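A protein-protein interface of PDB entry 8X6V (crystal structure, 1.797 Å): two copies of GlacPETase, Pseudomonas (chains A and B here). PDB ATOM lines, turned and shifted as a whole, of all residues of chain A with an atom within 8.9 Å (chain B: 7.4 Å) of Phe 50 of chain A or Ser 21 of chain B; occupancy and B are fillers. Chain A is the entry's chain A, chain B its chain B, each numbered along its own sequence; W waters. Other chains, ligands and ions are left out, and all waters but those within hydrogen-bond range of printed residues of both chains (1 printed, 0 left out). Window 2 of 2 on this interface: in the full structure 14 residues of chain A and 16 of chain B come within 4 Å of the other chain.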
ATOM      1  N   THR A  47      -4.119  21.020  30.662  1.00  0.00           N
ATOM      2  CA  THR A  47      -5.519  21.201  30.321  1.00  0.00           C
ATOM      3  C   THR A  47      -5.616  21.822  28.944  1.00  0.00           C
ATOM      4  O   THR A  47      -4.670  22.446  28.456  1.00  0.00           O
ATOM      5  CB  THR A  47      -6.294  22.094  31.315  1.00  0.00           C
ATOM      6  OG1 THR A  47      -6.015  23.481  31.056  1.00  0.00           O
ATOM      7  CG2 THR A  47      -5.953  21.753  32.745  1.00  0.00           C
ATOM      8  N   GLY A  48      -6.770  21.605  28.324  1.00  0.00           N
ATOM      9  CA  GLY A  48      -7.225  22.414  27.216  1.00  0.00           C
ATOM     10  C   GLY A  48      -7.873  23.687  27.729  1.00  0.00           C
ATOM     11  O   GLY A  48      -7.616  24.140  28.850  1.00  0.00           O
ATOM     12  N   GLY A  49      -8.738  24.269  26.889  1.00  0.00           N
ATOM     13  CA  GLY A  49      -9.438  25.493  27.235  1.00  0.00           C
ATOM     14  C   GLY A  49     -10.947  25.361  27.127  1.00  0.00           C
ATOM     15  O   GLY A  49     -11.487  24.261  27.261  1.00  0.00           O
ATOM     16  N   PHE A  50     -11.628  26.482  26.875  1.00  0.00           N
ATOM     17  CA  PHE A  50     -13.084  26.513  26.720  1.00  0.00           C
ATOM     18  C   PHE A  50     -13.557  25.485  25.697  1.00  0.00           C
ATOM     19  O   PHE A  50     -13.065  25.449  24.562  1.00  0.00           O
ATOM     20  CB  PHE A  50     -13.503  27.925  26.295  1.00  0.00           C
ATOM     21  CG  PHE A  50     -14.997  28.161  26.262  1.00  0.00           C
ATOM     22  CD1 PHE A  50     -15.731  27.897  25.118  1.00  0.00           C
ATOM     23  CD2 PHE A  50     -15.654  28.701  27.360  1.00  0.00           C
ATOM     24  CE1 PHE A  50     -17.104  28.158  25.075  1.00  0.00           C
ATOM     25  CE2 PHE A  50     -17.017  28.946  27.327  1.00  0.00           C
ATOM     26  CZ  PHE A  50     -17.741  28.675  26.185  1.00  0.00           C
ATOM     27  N   SER A  51     -14.493  24.635  26.128  1.00  0.00           N
ATOM     28  CA  SER A  51     -15.121  23.540  25.383  1.00  0.00           C
ATOM     29  C   SER A  51     -14.162  22.399  25.054  1.00  0.00           C
ATOM     30  O   SER A  51     -14.492  21.544  24.223  1.00  0.00           O
ATOM     31  CB  SER A  51     -15.797  24.035  24.094  1.00  0.00           C
ATOM     32  OG  SER A  51     -14.843  24.264  23.092  1.00  0.00           O
ATOM     33  N   ASN A  52     -12.991  22.343  25.678  1.00  0.00           N
ATOM     34  CA  ASN A  52     -12.069  21.241  25.452  1.00  0.00           C
ATOM     35  C   ASN A  52     -12.192  20.185  26.548  1.00  0.00           C
ATOM     36  O   ASN A  52     -12.500  20.488  27.705  1.00  0.00           O
ATOM     37  CB  ASN A  52     -10.620  21.731  25.396  1.00  0.00           C
ATOM     38  CG  ASN A  52     -10.317  22.564  24.160  1.00  0.00           C
ATOM     39  OD1 ASN A  52      -9.589  23.546  24.243  1.00  0.00           O
ATOM     40  ND2 ASN A  52     -10.857  22.163  23.012  1.00  0.00           N
ATOM     41  N   THR A  53     -11.923  18.939  26.176  1.00  0.00           N
ATOM     42  CA  THR A  53     -11.817  17.838  27.125  1.00  0.00           C
ATOM     43  C   THR A  53     -10.387  17.303  27.128  1.00  0.00           C
ATOM     44  O   THR A  53      -9.609  17.564  26.206  1.00  0.00           O
ATOM     45  CB  THR A  53     -12.802  16.711  26.784  1.00  0.00           C
ATOM     46  OG1 THR A  53     -12.423  16.099  25.543  1.00  0.00           O
ATOM     47  CG2 THR A  53     -14.214  17.260  26.667  1.00  0.00           C
ATOM     48  N   GLN A  56      -8.646  15.685  24.105  1.00  0.00           N
ATOM     49  CA  GLN A  56      -8.131  16.467  22.991  1.00  0.00           C
ATOM     50  C   GLN A  56      -6.698  16.923  23.182  1.00  0.00           C
ATOM     51  O   GLN A  56      -6.149  17.557  22.274  1.00  0.00           O
ATOM     52  CB  GLN A  56      -9.017  17.686  22.764  1.00  0.00           C
ATOM     53  CG  GLN A  56     -10.413  17.321  22.341  1.00  0.00           C
ATOM     54  CD  GLN A  56     -11.232  18.541  22.093  1.00  0.00           C
ATOM     55  OE1 GLN A  56     -11.660  19.194  23.033  1.00  0.00           O
ATOM     56  NE2 GLN A  56     -11.426  18.889  20.816  1.00  0.00           N
ATOM     57  N   PRO A  76     -11.959  20.079  33.079  1.00  0.00           N
ATOM     58  CA  PRO A  76     -12.425  20.881  34.217  1.00  0.00           C
ATOM     59  C   PRO A  76     -13.867  20.553  34.572  1.00  0.00           C
ATOM     60  O   PRO A  76     -14.600  19.931  33.803  1.00  0.00           O
ATOM     61  CB  PRO A  76     -12.293  22.320  33.706  1.00  0.00           C
ATOM     62  CG  PRO A  76     -12.461  22.191  32.228  1.00  0.00           C
ATOM     63  CD  PRO A  76     -11.725  20.914  31.888  1.00  0.00           C
ATOM     64  N   ASN A  78     -16.294  22.615  34.618  1.00  0.00           N
ATOM     65  CA  ASN A  78     -17.170  23.311  33.680  1.00  0.00           C
ATOM     66  C   ASN A  78     -16.337  23.679  32.458  1.00  0.00           C
ATOM     67  O   ASN A  78     -15.608  24.674  32.487  1.00  0.00           O
ATOM     68  CB  ASN A  78     -17.787  24.551  34.329  1.00  0.00           C
ATOM     69  CG  ASN A  78     -18.741  25.288  33.404  1.00  0.00           C
ATOM     70  OD1 ASN A  78     -19.027  24.834  32.303  1.00  0.00           O
ATOM     71  ND2 ASN A  78     -19.233  26.432  33.857  1.00  0.00           N
ATOM     72  N   ILE A  79     -16.454  22.897  31.381  1.00  0.00           N
ATOM     73  CA  ILE A  79     -15.698  23.222  30.173  1.00  0.00           C
ATOM     74  C   ILE A  79     -16.186  24.495  29.509  1.00  0.00           C
ATOM     75  O   ILE A  79     -15.489  25.036  28.647  1.00  0.00           O
ATOM     76  CB  ILE A  79     -15.718  22.067  29.151  1.00  0.00           C
ATOM     77  CG1 ILE A  79     -17.107  21.873  28.550  1.00  0.00           C
ATOM     78  CG2 ILE A  79     -15.231  20.786  29.790  1.00  0.00           C
ATOM     79  CD1 ILE A  79     -17.077  21.032  27.273  1.00  0.00           C
ATOM     80  N   PHE A  80     -17.353  25.001  29.899  1.00  0.00           N
ATOM     81  CA  PHE A  80     -17.868  26.248  29.350  1.00  0.00           C
ATOM     82  C   PHE A  80     -17.760  27.392  30.357  1.00  0.00           C
ATOM     83  O   PHE A  80     -18.525  28.361  30.297  1.00  0.00           O
ATOM     84  CB  PHE A  80     -19.306  26.054  28.879  1.00  0.00           C
ATOM     85  CG  PHE A  80     -19.478  24.905  27.916  1.00  0.00           C
ATOM     86  CD1 PHE A  80     -18.960  24.977  26.632  1.00  0.00           C
ATOM     87  CD2 PHE A  80     -20.166  23.765  28.288  1.00  0.00           C
ATOM     88  CE1 PHE A  80     -19.121  23.932  25.740  1.00  0.00           C
ATOM     89  CE2 PHE A  80     -20.332  22.713  27.400  1.00  0.00           C
ATOM     90  CZ  PHE A  80     -19.813  22.804  26.119  1.00  0.00           C
ATOM     91  N   GLY A  81     -16.800  27.296  31.278  1.00  0.00           N
ATOM     92  CA  GLY A  81     -16.603  28.287  32.314  1.00  0.00           C
ATOM     93  C   GLY A  81     -15.697  29.432  31.898  1.00  0.00           C
ATOM     94  O   GLY A  81     -15.526  29.739  30.715  1.00  0.00           O
ATOM     95  N   ALA A  82     -15.129  30.081  32.899  1.00  0.00           N
ATOM     96  CA  ALA A  82     -14.192  31.180  32.755  1.00  0.00           C
ATOM     97  C   ALA A  82     -12.790  30.735  33.169  1.00  0.00           C
ATOM     98  O   ALA A  82     -12.618  29.674  33.778  1.00  0.00           O
ATOM     99  CB  ALA A  82     -14.649  32.371  33.610  1.00  0.00           C
ATOM    100  N   PRO A  83     -11.760  31.526  32.855  1.00  0.00           N
ATOM    101  CA  PRO A  83     -10.383  31.097  33.177  1.00  0.00           C
ATOM    102  C   PRO A  83     -10.148  30.704  34.635  1.00  0.00           C
ATOM    103  O   PRO A  83      -9.309  29.836  34.881  1.00  0.00           O
ATOM    104  CB  PRO A  83      -9.543  32.320  32.786  1.00  0.00           C
ATOM    105  CG  PRO A  83     -10.296  32.938  31.674  1.00  0.00           C
ATOM    106  CD  PRO A  83     -11.765  32.704  31.964  1.00  0.00           C
ATOM    107  N   TRP A  86     -10.271  26.978  35.148  1.00  0.00           N
ATOM    108  CA  TRP A  86      -9.074  26.208  34.825  1.00  0.00           C
ATOM    109  C   TRP A  86      -7.971  26.434  35.851  1.00  0.00           C
ATOM    110  O   TRP A  86      -7.157  25.532  36.099  1.00  0.00           O
ATOM    111  CB  TRP A  86      -8.599  26.560  33.410  1.00  0.00           C
ATOM    112  CG  TRP A  86      -9.412  25.861  32.365  1.00  0.00           C
ATOM    113  CD1 TRP A  86      -9.136  24.645  31.788  1.00  0.00           C
ATOM    114  CD2 TRP A  86     -10.642  26.311  31.784  1.00  0.00           C
ATOM    115  NE1 TRP A  86     -10.124  24.320  30.886  1.00  0.00           N
ATOM    116  CE2 TRP A  86     -11.059  25.323  30.867  1.00  0.00           C
ATOM    117  CE3 TRP A  86     -11.438  27.452  31.955  1.00  0.00           C
ATOM    118  CZ2 TRP A  86     -12.230  25.439  30.124  1.00  0.00           C
ATOM    119  CZ3 TRP A  86     -12.606  27.567  31.210  1.00  0.00           C
ATOM    120  CH2 TRP A  86     -12.987  26.566  30.301  1.00  0.00           C
ATOM    121  N   PHE A 122      -3.710  25.272  27.670  1.00  0.00           N
ATOM    122  CA  PHE A 122      -4.005  25.885  26.375  1.00  0.00           C
ATOM    123  C   PHE A 122      -5.182  26.847  26.489  1.00  0.00           C
ATOM    124  O   PHE A 122      -6.215  26.496  27.064  1.00  0.00           O
ATOM    125  CB  PHE A 122      -4.328  24.797  25.345  1.00  0.00           C
ATOM    126  CG  PHE A 122      -5.023  25.302  24.113  1.00  0.00           C
ATOM    127  CD1 PHE A 122      -4.416  26.239  23.296  1.00  0.00           C
ATOM    128  CD2 PHE A 122      -6.286  24.829  23.774  1.00  0.00           C
ATOM    129  CE1 PHE A 122      -5.063  26.708  22.144  1.00  0.00           C
ATOM    130  CE2 PHE A 122      -6.936  25.279  22.626  1.00  0.00           C
ATOM    131  CZ  PHE A 122      -6.318  26.227  21.806  1.00  0.00           C
ATOM    132  N   SER A 123      -5.034  28.049  25.908  1.00  0.00           N
ATOM    133  CA  SER A 123      -6.121  29.033  25.781  1.00  0.00           C
ATOM    134  C   SER A 123      -6.623  29.397  27.187  1.00  0.00           C
ATOM    135  O   SER A 123      -5.818  29.832  28.015  1.00  0.00           O
ATOM    136  CB  SER A 123      -7.167  28.476  24.817  1.00  0.00           C
ATOM    137  OG  SER A 123      -8.064  29.484  24.369  1.00  0.00           O
ATOM    138  N   MET A 124      -7.914  29.231  27.498  1.00  0.00           N
ATOM    139  CA  MET A 124      -8.354  29.538  28.859  1.00  0.00           C
ATOM    140  C   MET A 124      -7.653  28.665  29.889  1.00  0.00           C
ATOM    141  O   MET A 124      -7.555  29.065  31.052  1.00  0.00           O
ATOM    142  CB  MET A 124      -9.878  29.390  28.995  1.00  0.00           C
ATOM    143  CG  MET A 124     -10.648  30.572  28.424  1.00  0.00           C
ATOM    144  SD  MET A 124     -12.363  30.544  28.987  1.00  0.00           S
ATOM    145  CE  MET A 124     -12.969  31.996  28.138  1.00  0.00           C
ATOM    146  N   GLY A 125      -7.149  27.493  29.494  1.00  0.00           N
ATOM    147  CA  GLY A 125      -6.313  26.725  30.407  1.00  0.00           C
ATOM    148  C   GLY A 125      -4.942  27.334  30.602  1.00  0.00           C
ATOM    149  O   GLY A 125      -4.310  27.107  31.639  1.00  0.00           O
ATOM    150  N   GLY A 126      -4.476  28.106  29.622  1.00  0.00           N
ATOM    151  CA  GLY A 126      -3.238  28.847  29.736  1.00  0.00           C
ATOM    152  C   GLY A 126      -3.411  30.065  30.612  1.00  0.00           C
ATOM    153  O   GLY A 126      -2.516  30.408  31.384  1.00  0.00           O
ATOM    154  N   PHE A 149      -5.506  32.687  27.177  1.00  0.00           N
ATOM    155  CA  PHE A 149      -6.641  33.598  27.072  1.00  0.00           C
ATOM    156  C   PHE A 149      -7.083  33.926  28.494  1.00  0.00           C
ATOM    157  O   PHE A 149      -7.576  33.047  29.203  1.00  0.00           O
ATOM    158  CB  PHE A 149      -7.768  32.950  26.265  1.00  0.00           C
ATOM    159  CG  PHE A 149      -8.939  33.865  25.998  1.00  0.00           C
ATOM    160  CD1 PHE A 149      -9.925  34.051  26.960  1.00  0.00           C
ATOM    161  CD2 PHE A 149      -9.054  34.524  24.789  1.00  0.00           C
ATOM    162  CE1 PHE A 149     -11.002  34.893  26.721  1.00  0.00           C
ATOM    163  CE2 PHE A 149     -10.130  35.365  24.543  1.00  0.00           C
ATOM    164  CZ  PHE A 149     -11.104  35.547  25.514  1.00  0.00           C
ATOM    165  N   VAL A 174      -7.931  34.202  18.331  1.00  0.00           N
ATOM    166  CA  VAL A 174      -8.647  34.069  19.598  1.00  0.00           C
ATOM    167  C   VAL A 174      -7.731  34.555  20.711  1.00  0.00           C
ATOM    168  O   VAL A 174      -8.089  35.450  21.487  1.00  0.00           O
ATOM    169  CB  VAL A 174      -9.098  32.619  19.854  1.00  0.00           C
ATOM    170  CG1 VAL A 174      -9.734  32.503  21.225  1.00  0.00           C
ATOM    171  CG2 VAL A 174     -10.065  32.142  18.770  1.00  0.00           C
ATOM    172  N   HIS A 203      -4.848  29.160  16.361  1.00  0.00           N
ATOM    173  CA  HIS A 203      -5.247  28.864  17.736  1.00  0.00           C
ATOM    174  C   HIS A 203      -5.422  27.371  17.965  1.00  0.00           C
ATOM    175  O   HIS A 203      -4.980  26.837  18.988  1.00  0.00           O
ATOM    176  CB  HIS A 203      -6.543  29.592  18.079  1.00  0.00           C
ATOM    177  CG  HIS A 203      -6.851  29.590  19.546  1.00  0.00           C
ATOM    178  ND1 HIS A 203      -6.006  30.154  20.476  1.00  0.00           N
ATOM    179  CD2 HIS A 203      -7.901  29.093  20.243  1.00  0.00           C
ATOM    180  CE1 HIS A 203      -6.533  30.026  21.683  1.00  0.00           C
ATOM    181  NE2 HIS A 203      -7.675  29.373  21.569  1.00  0.00           N
ATOM    182  N   LEU A 204      -6.037  26.672  17.017  1.00  0.00           N
ATOM    183  CA  LEU A 204      -6.323  25.260  17.238  1.00  0.00           C
ATOM    184  C   LEU A 204      -5.134  24.346  16.897  1.00  0.00           C
ATOM    185  O   LEU A 204      -5.317  23.132  16.759  1.00  0.00           O
ATOM    186  CB  LEU A 204      -7.581  24.862  16.457  1.00  0.00           C
ATOM    187  CG  LEU A 204      -8.802  25.651  16.970  1.00  0.00           C
ATOM    188  CD1 LEU A 204     -10.077  25.284  16.223  1.00  0.00           C
ATOM    189  CD2 LEU A 204      -8.973  25.425  18.442  1.00  0.00           C
ATOM    190  N   ILE A 207      -4.503  21.667  20.005  1.00  0.00           N
ATOM    191  CA  ILE A 207      -5.314  20.488  20.282  1.00  0.00           C
ATOM    192  C   ILE A 207      -4.993  19.432  19.220  1.00  0.00           C
ATOM    193  O   ILE A 207      -4.257  19.690  18.272  1.00  0.00           O
ATOM    194  CB  ILE A 207      -6.821  20.812  20.333  1.00  0.00           C
ATOM    195  CG1 ILE A 207      -7.277  21.441  19.016  1.00  0.00           C
ATOM    196  CG2 ILE A 207      -7.105  21.734  21.505  1.00  0.00           C
ATOM    197  CD1 ILE A 207      -8.782  21.650  18.950  1.00  0.00           C
ATOM    198  N   THR B  17     -28.521  22.134  19.923  1.00  0.00           N
ATOM    199  CA  THR B  17     -27.559  23.223  19.993  1.00  0.00           C
ATOM    200  C   THR B  17     -26.873  23.312  21.345  1.00  0.00           C
ATOM    201  O   THR B  17     -25.872  24.028  21.463  1.00  0.00           O
ATOM    202  CB  THR B  17     -28.232  24.574  19.689  1.00  0.00           C
ATOM    203  OG1 THR B  17     -29.314  24.787  20.601  1.00  0.00           O
ATOM    204  CG2 THR B  17     -28.774  24.618  18.254  1.00  0.00           C
ATOM    205  N   SER B  18     -27.367  22.599  22.358  1.00  0.00           N
ATOM    206  CA  SER B  18     -26.830  22.716  23.704  1.00  0.00           C
ATOM    207  C   SER B  18     -25.476  22.030  23.788  1.00  0.00           C
ATOM    208  O   SER B  18     -25.344  20.858  23.425  1.00  0.00           O
ATOM    209  CB  SER B  18     -27.800  22.098  24.713  1.00  0.00           C
ATOM    210  OG  SER B  18     -27.111  21.574  25.834  1.00  0.00           O
ATOM    211  N   GLY B  19     -24.480  22.759  24.283  1.00  0.00           N
ATOM    212  CA  GLY B  19     -23.131  22.246  24.398  1.00  0.00           C
ATOM    213  C   GLY B  19     -22.229  22.522  23.218  1.00  0.00           C
ATOM    214  O   GLY B  19     -21.103  22.012  23.187  1.00  0.00           O
ATOM    215  N   LEU B  20     -22.668  23.324  22.253  1.00  0.00           N
ATOM    216  CA  LEU B  20     -21.903  23.510  21.026  1.00  0.00           C
ATOM    217  C   LEU B  20     -21.114  24.811  20.998  1.00  0.00           C
ATOM    218  O   LEU B  20     -20.483  25.114  19.973  1.00  0.00           O
ATOM    219  CB  LEU B  20     -22.839  23.431  19.812  1.00  0.00           C
ATOM    220  CG  LEU B  20     -23.491  22.056  19.632  1.00  0.00           C
ATOM    221  CD1 LEU B  20     -24.339  22.025  18.360  1.00  0.00           C
ATOM    222  CD2 LEU B  20     -22.455  20.924  19.616  1.00  0.00           C
ATOM    223  N   SER B  21     -21.117  25.577  22.091  1.00  0.00           N
ATOM    224  CA  SER B  21     -20.368  26.826  22.134  1.00  0.00           C
ATOM    225  C   SER B  21     -18.887  26.566  21.881  1.00  0.00           C
ATOM    226  O   SER B  21     -18.349  25.526  22.264  1.00  0.00           O
ATOM    227  CB  SER B  21     -20.534  27.510  23.494  1.00  0.00           C
ATOM    228  OG  SER B  21     -21.818  28.105  23.606  1.00  0.00           O
ATOM    229  N   SER B  22     -18.234  27.532  21.233  1.00  0.00           N
ATOM    230  CA  SER B  22     -16.793  27.495  21.014  1.00  0.00           C
ATOM    231  C   SER B  22     -16.285  28.924  20.896  1.00  0.00           C
ATOM    232  O   SER B  22     -16.984  29.804  20.394  1.00  0.00           O
ATOM    233  CB  SER B  22     -16.423  26.697  19.760  1.00  0.00           C
ATOM    234  OG  SER B  22     -15.107  27.027  19.306  1.00  0.00           O
ATOM    235  N   LEU B  23     -15.059  29.158  21.376  1.00  0.00           N
ATOM    236  CA  LEU B  23     -14.474  30.484  21.207  1.00  0.00           C
ATOM    237  C   LEU B  23     -14.121  30.788  19.758  1.00  0.00           C
ATOM    238  O   LEU B  23     -13.867  31.951  19.432  1.00  0.00           O
ATOM    239  CB  LEU B  23     -13.213  30.629  22.060  1.00  0.00           C
ATOM    240  CG  LEU B  23     -13.325  30.687  23.577  1.00  0.00           C
ATOM    241  CD1 LEU B  23     -11.975  31.098  24.180  1.00  0.00           C
ATOM    242  CD2 LEU B  23     -14.426  31.628  24.013  1.00  0.00           C
ATOM    243  N   SER B  24     -14.096  29.781  18.890  1.00  0.00           N
ATOM    244  CA  SER B  24     -13.637  29.950  17.522  1.00  0.00           C
ATOM    245  C   SER B  24     -14.765  30.171  16.521  1.00  0.00           C
ATOM    246  O   SER B  24     -14.478  30.425  15.346  1.00  0.00           O
ATOM    247  CB  SER B  24     -12.805  28.734  17.106  1.00  0.00           C
ATOM    248  OG  SER B  24     -11.577  28.725  17.815  1.00  0.00           O
ATOM    249  N   TYR B  25     -16.028  30.103  16.945  1.00  0.00           N
ATOM    250  CA  TYR B  25     -17.125  30.499  16.067  1.00  0.00           C
ATOM    251  C   TYR B  25     -18.247  31.093  16.914  1.00  0.00           C
ATOM    252  O   TYR B  25     -18.174  31.110  18.144  1.00  0.00           O
ATOM    253  CB  TYR B  25     -17.613  29.329  15.202  1.00  0.00           C
ATOM    254  CG  TYR B  25     -18.012  28.041  15.924  1.00  0.00           C
ATOM    255  CD1 TYR B  25     -19.062  28.016  16.850  1.00  0.00           C
ATOM    256  CD2 TYR B  25     -17.373  26.843  15.633  1.00  0.00           C
ATOM    257  CE1 TYR B  25     -19.428  26.834  17.477  1.00  0.00           C
ATOM    258  CE2 TYR B  25     -17.729  25.666  16.248  1.00  0.00           C
ATOM    259  CZ  TYR B  25     -18.759  25.665  17.174  1.00  0.00           C
ATOM    260  OH  TYR B  25     -19.115  24.482  17.772  1.00  0.00           O
ATOM    261  N   ALA B  26     -19.283  31.602  16.237  1.00  0.00           N
ATOM    262  CA  ALA B  26     -20.357  32.299  16.943  1.00  0.00           C
ATOM    263  C   ALA B  26     -21.404  31.327  17.475  1.00  0.00           C
ATOM    264  O   ALA B  26     -21.844  31.449  18.625  1.00  0.00           O
ATOM    265  CB  ALA B  26     -21.012  33.342  16.029  1.00  0.00           C
ATOM    266  N   SER B  27     -21.824  30.362  16.657  1.00  0.00           N
ATOM    267  CA  SER B  27     -22.860  29.422  17.072  1.00  0.00           C
ATOM    268  C   SER B  27     -22.852  28.235  16.121  1.00  0.00           C
ATOM    269  O   SER B  27     -22.326  28.316  15.006  1.00  0.00           O
ATOM    270  CB  SER B  27     -24.250  30.082  17.104  1.00  0.00           C
ATOM    271  OG  SER B  27     -24.636  30.553  15.817  1.00  0.00           O
ATOM    272  N   ALA B  28     -23.443  27.129  16.574  1.00  0.00           N
ATOM    273  CA  ALA B  28     -23.437  25.904  15.787  1.00  0.00           C
ATOM    274  C   ALA B  28     -24.704  25.107  16.052  1.00  0.00           C
ATOM    275  O   ALA B  28     -25.366  25.279  17.077  1.00  0.00           O
ATOM    276  CB  ALA B  28     -22.190  25.056  16.086  1.00  0.00           C
ATOM    277  N   LYS B  96     -14.972  20.290  17.743  1.00  0.00           N
ATOM    278  CA  LYS B  96     -16.197  20.110  18.516  1.00  0.00           C
ATOM    279  C   LYS B  96     -16.746  18.697  18.374  1.00  0.00           C
ATOM    280  O   LYS B  96     -17.184  18.095  19.361  1.00  0.00           O
ATOM    281  CB  LYS B  96     -17.235  21.143  18.083  1.00  0.00           C
ATOM    282  CG  LYS B  96     -18.598  20.985  18.750  1.00  0.00           C
ATOM    283  CD  LYS B  96     -18.483  20.981  20.269  1.00  0.00           C
ATOM    284  CE  LYS B  96     -18.288  22.389  20.838  1.00  0.00           C
ATOM    285  NZ  LYS B  96     -18.524  22.424  22.337  1.00  0.00           N
ATOM    286  N   SER B  99     -14.645  16.527  20.478  1.00  0.00           N
ATOM    287  CA  SER B  99     -15.000  16.827  21.861  1.00  0.00           C
ATOM    288  C   SER B  99     -16.333  16.192  22.234  1.00  0.00           C
ATOM    289  O   SER B  99     -16.456  15.552  23.287  1.00  0.00           O
ATOM    290  CB  SER B  99     -15.048  18.344  22.058  1.00  0.00           C
ATOM    291  OG  SER B  99     -15.375  18.696  23.393  1.00  0.00           O
ATOM    292  N   GLU B 100     -17.347  16.354  21.371  1.00  0.00           N
ATOM    293  CA  GLU B 100     -18.657  15.767  21.641  1.00  0.00           C
ATOM    294  C   GLU B 100     -18.598  14.246  21.720  1.00  0.00           C
ATOM    295  O   GLU B 100     -19.389  13.637  22.449  1.00  0.00           O
ATOM    296  CB  GLU B 100     -19.665  16.194  20.572  1.00  0.00           C
ATOM    297  CG  GLU B 100     -20.063  17.651  20.649  1.00  0.00           C
ATOM    298  CD  GLU B 100     -20.887  17.953  21.878  1.00  0.00           C
ATOM    299  OE1 GLU B 100     -22.109  17.702  21.852  1.00  0.00           O
ATOM    300  OE2 GLU B 100     -20.306  18.430  22.873  1.00  0.00           O
HETATM  301  O   HOH W   1     -13.254  27.056  22.090  1.00  0.00           O
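O of Ser 51 of chain A sits at hydrogen-bond distance from OG of Ser 99 of chain B (3.1 Å).
Of chain B, only Ser 21 (3.8 Å) and Leu 23 (3.9 Å) come within 4 Å of Phe 50 of chain A. Of the printed residues of chain B, Gln 56 of chain A touches Ser 99 (3.6 Å). Printed residues of chain B within 4 Å of Val 174 of chain A: Leu 23 (3.9 Å) and Ser 24 (3.9 Å). No residue of chain A comes within 4 Å of Ser 22 of chain B. Printed residues of chain A within 4 Å of Leu 23 of chain B: Phe 50 (3.9 Å) and Val 174 (3.9 Å). Printed residues of chain A within 4 Å of Ser 99 of chain B: Ser 51, Thr 53 and Gln 56. The nearest residue of chain B that does not touch Phe 50 of chain A is Ser 22 of chain B (4.1 Å). The nearest residue of chain A that does not touch Ser 21 of chain B is Ile 79 of chain A (6.8 Å). The nearest printed residue of chain A that does not touch Ser 24 of chain B is Leu 204 of chain A (4.1 Å).
Water W1 lies within hydrogen-bond range of the backbone NH of Leu 23 of chain B (2.9 Å), the backbone carbonyl oxygen of Phe 50 of chain A (3.0 Å), the side-chain hydroxyl of Ser 22 of chain B (3.3 Å) and the side-chain hydroxyl of Ser 51 of chain A (3.4 Å).
The backbone carbonyl oxygen of Ile 79 of chain A is in hydrogen-bond range of the backbone NH of Ser 51 of chain A (2.7 Å). OD1 of Asn 78 of chain A lies within hydrogen-bond range of N of Phe 80 of chain A (2.9 Å). The backbone carbonyl oxygen (O) of Gly 19 of chain B lies within hydrogen-bond range of the side-chain amino group (NZ) of Lys 96 of chain B (2.7 Å). The side-chain hydroxyl of Ser 22 of chain B lies within hydrogen-bond range of the backbone NH of Ser 24 of chain B (3.0 Å). The backbone NH of Thr 53 of chain A lies within hydrogen-bond range of the side-chain amide oxygen of Gln 56 of chain A, 3.2 Å away. NZ of Lys 96 of chain B is in hydrogen-bond range of O of Ser 21 of chain B, 3.1 Å away.
No position is printed for both chains.
Phe 50 of chain A touches Ser 21 of chain B. Phe 50 of chain A touches Leu 23 of chain B. Ser 51 of chain A touches Ser 21 of chain B. Ser 51 of chain A touches Lys 96 of chain B. Thr 53 of chain A touches Ser 99 of chain B. Gln 56 of chain A touches Ser 99 of chain B. O of Gly 19 of chain B touches CZ of Phe 80 of chain A, at 3.3 Å. Phe 80 of chain A touches Ser 21 of chain B. Phe 80 of chain A touches Lys 96 of chain B (CE1 to NZ, 3.8 Å). Val 174 of chain A touches Ser 24 of chain B.
Hydrophobic or aromatic side chains of chain A within 4 Å of the printed part of chain B: Phe 50, Phe 80 and Val 174. Printed residues of chain B that touch a printed residue of chain A: Gly 19, Ser 21, Leu 23, Ser 24, Lys 96 and Ser 99. Among the printed residues, 12 pairs touch across the chains. Among the printed residues, no Asp or Glu carboxylate lies within 4 Å of a Lys or Arg side-chain nitrogen of the other chain.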
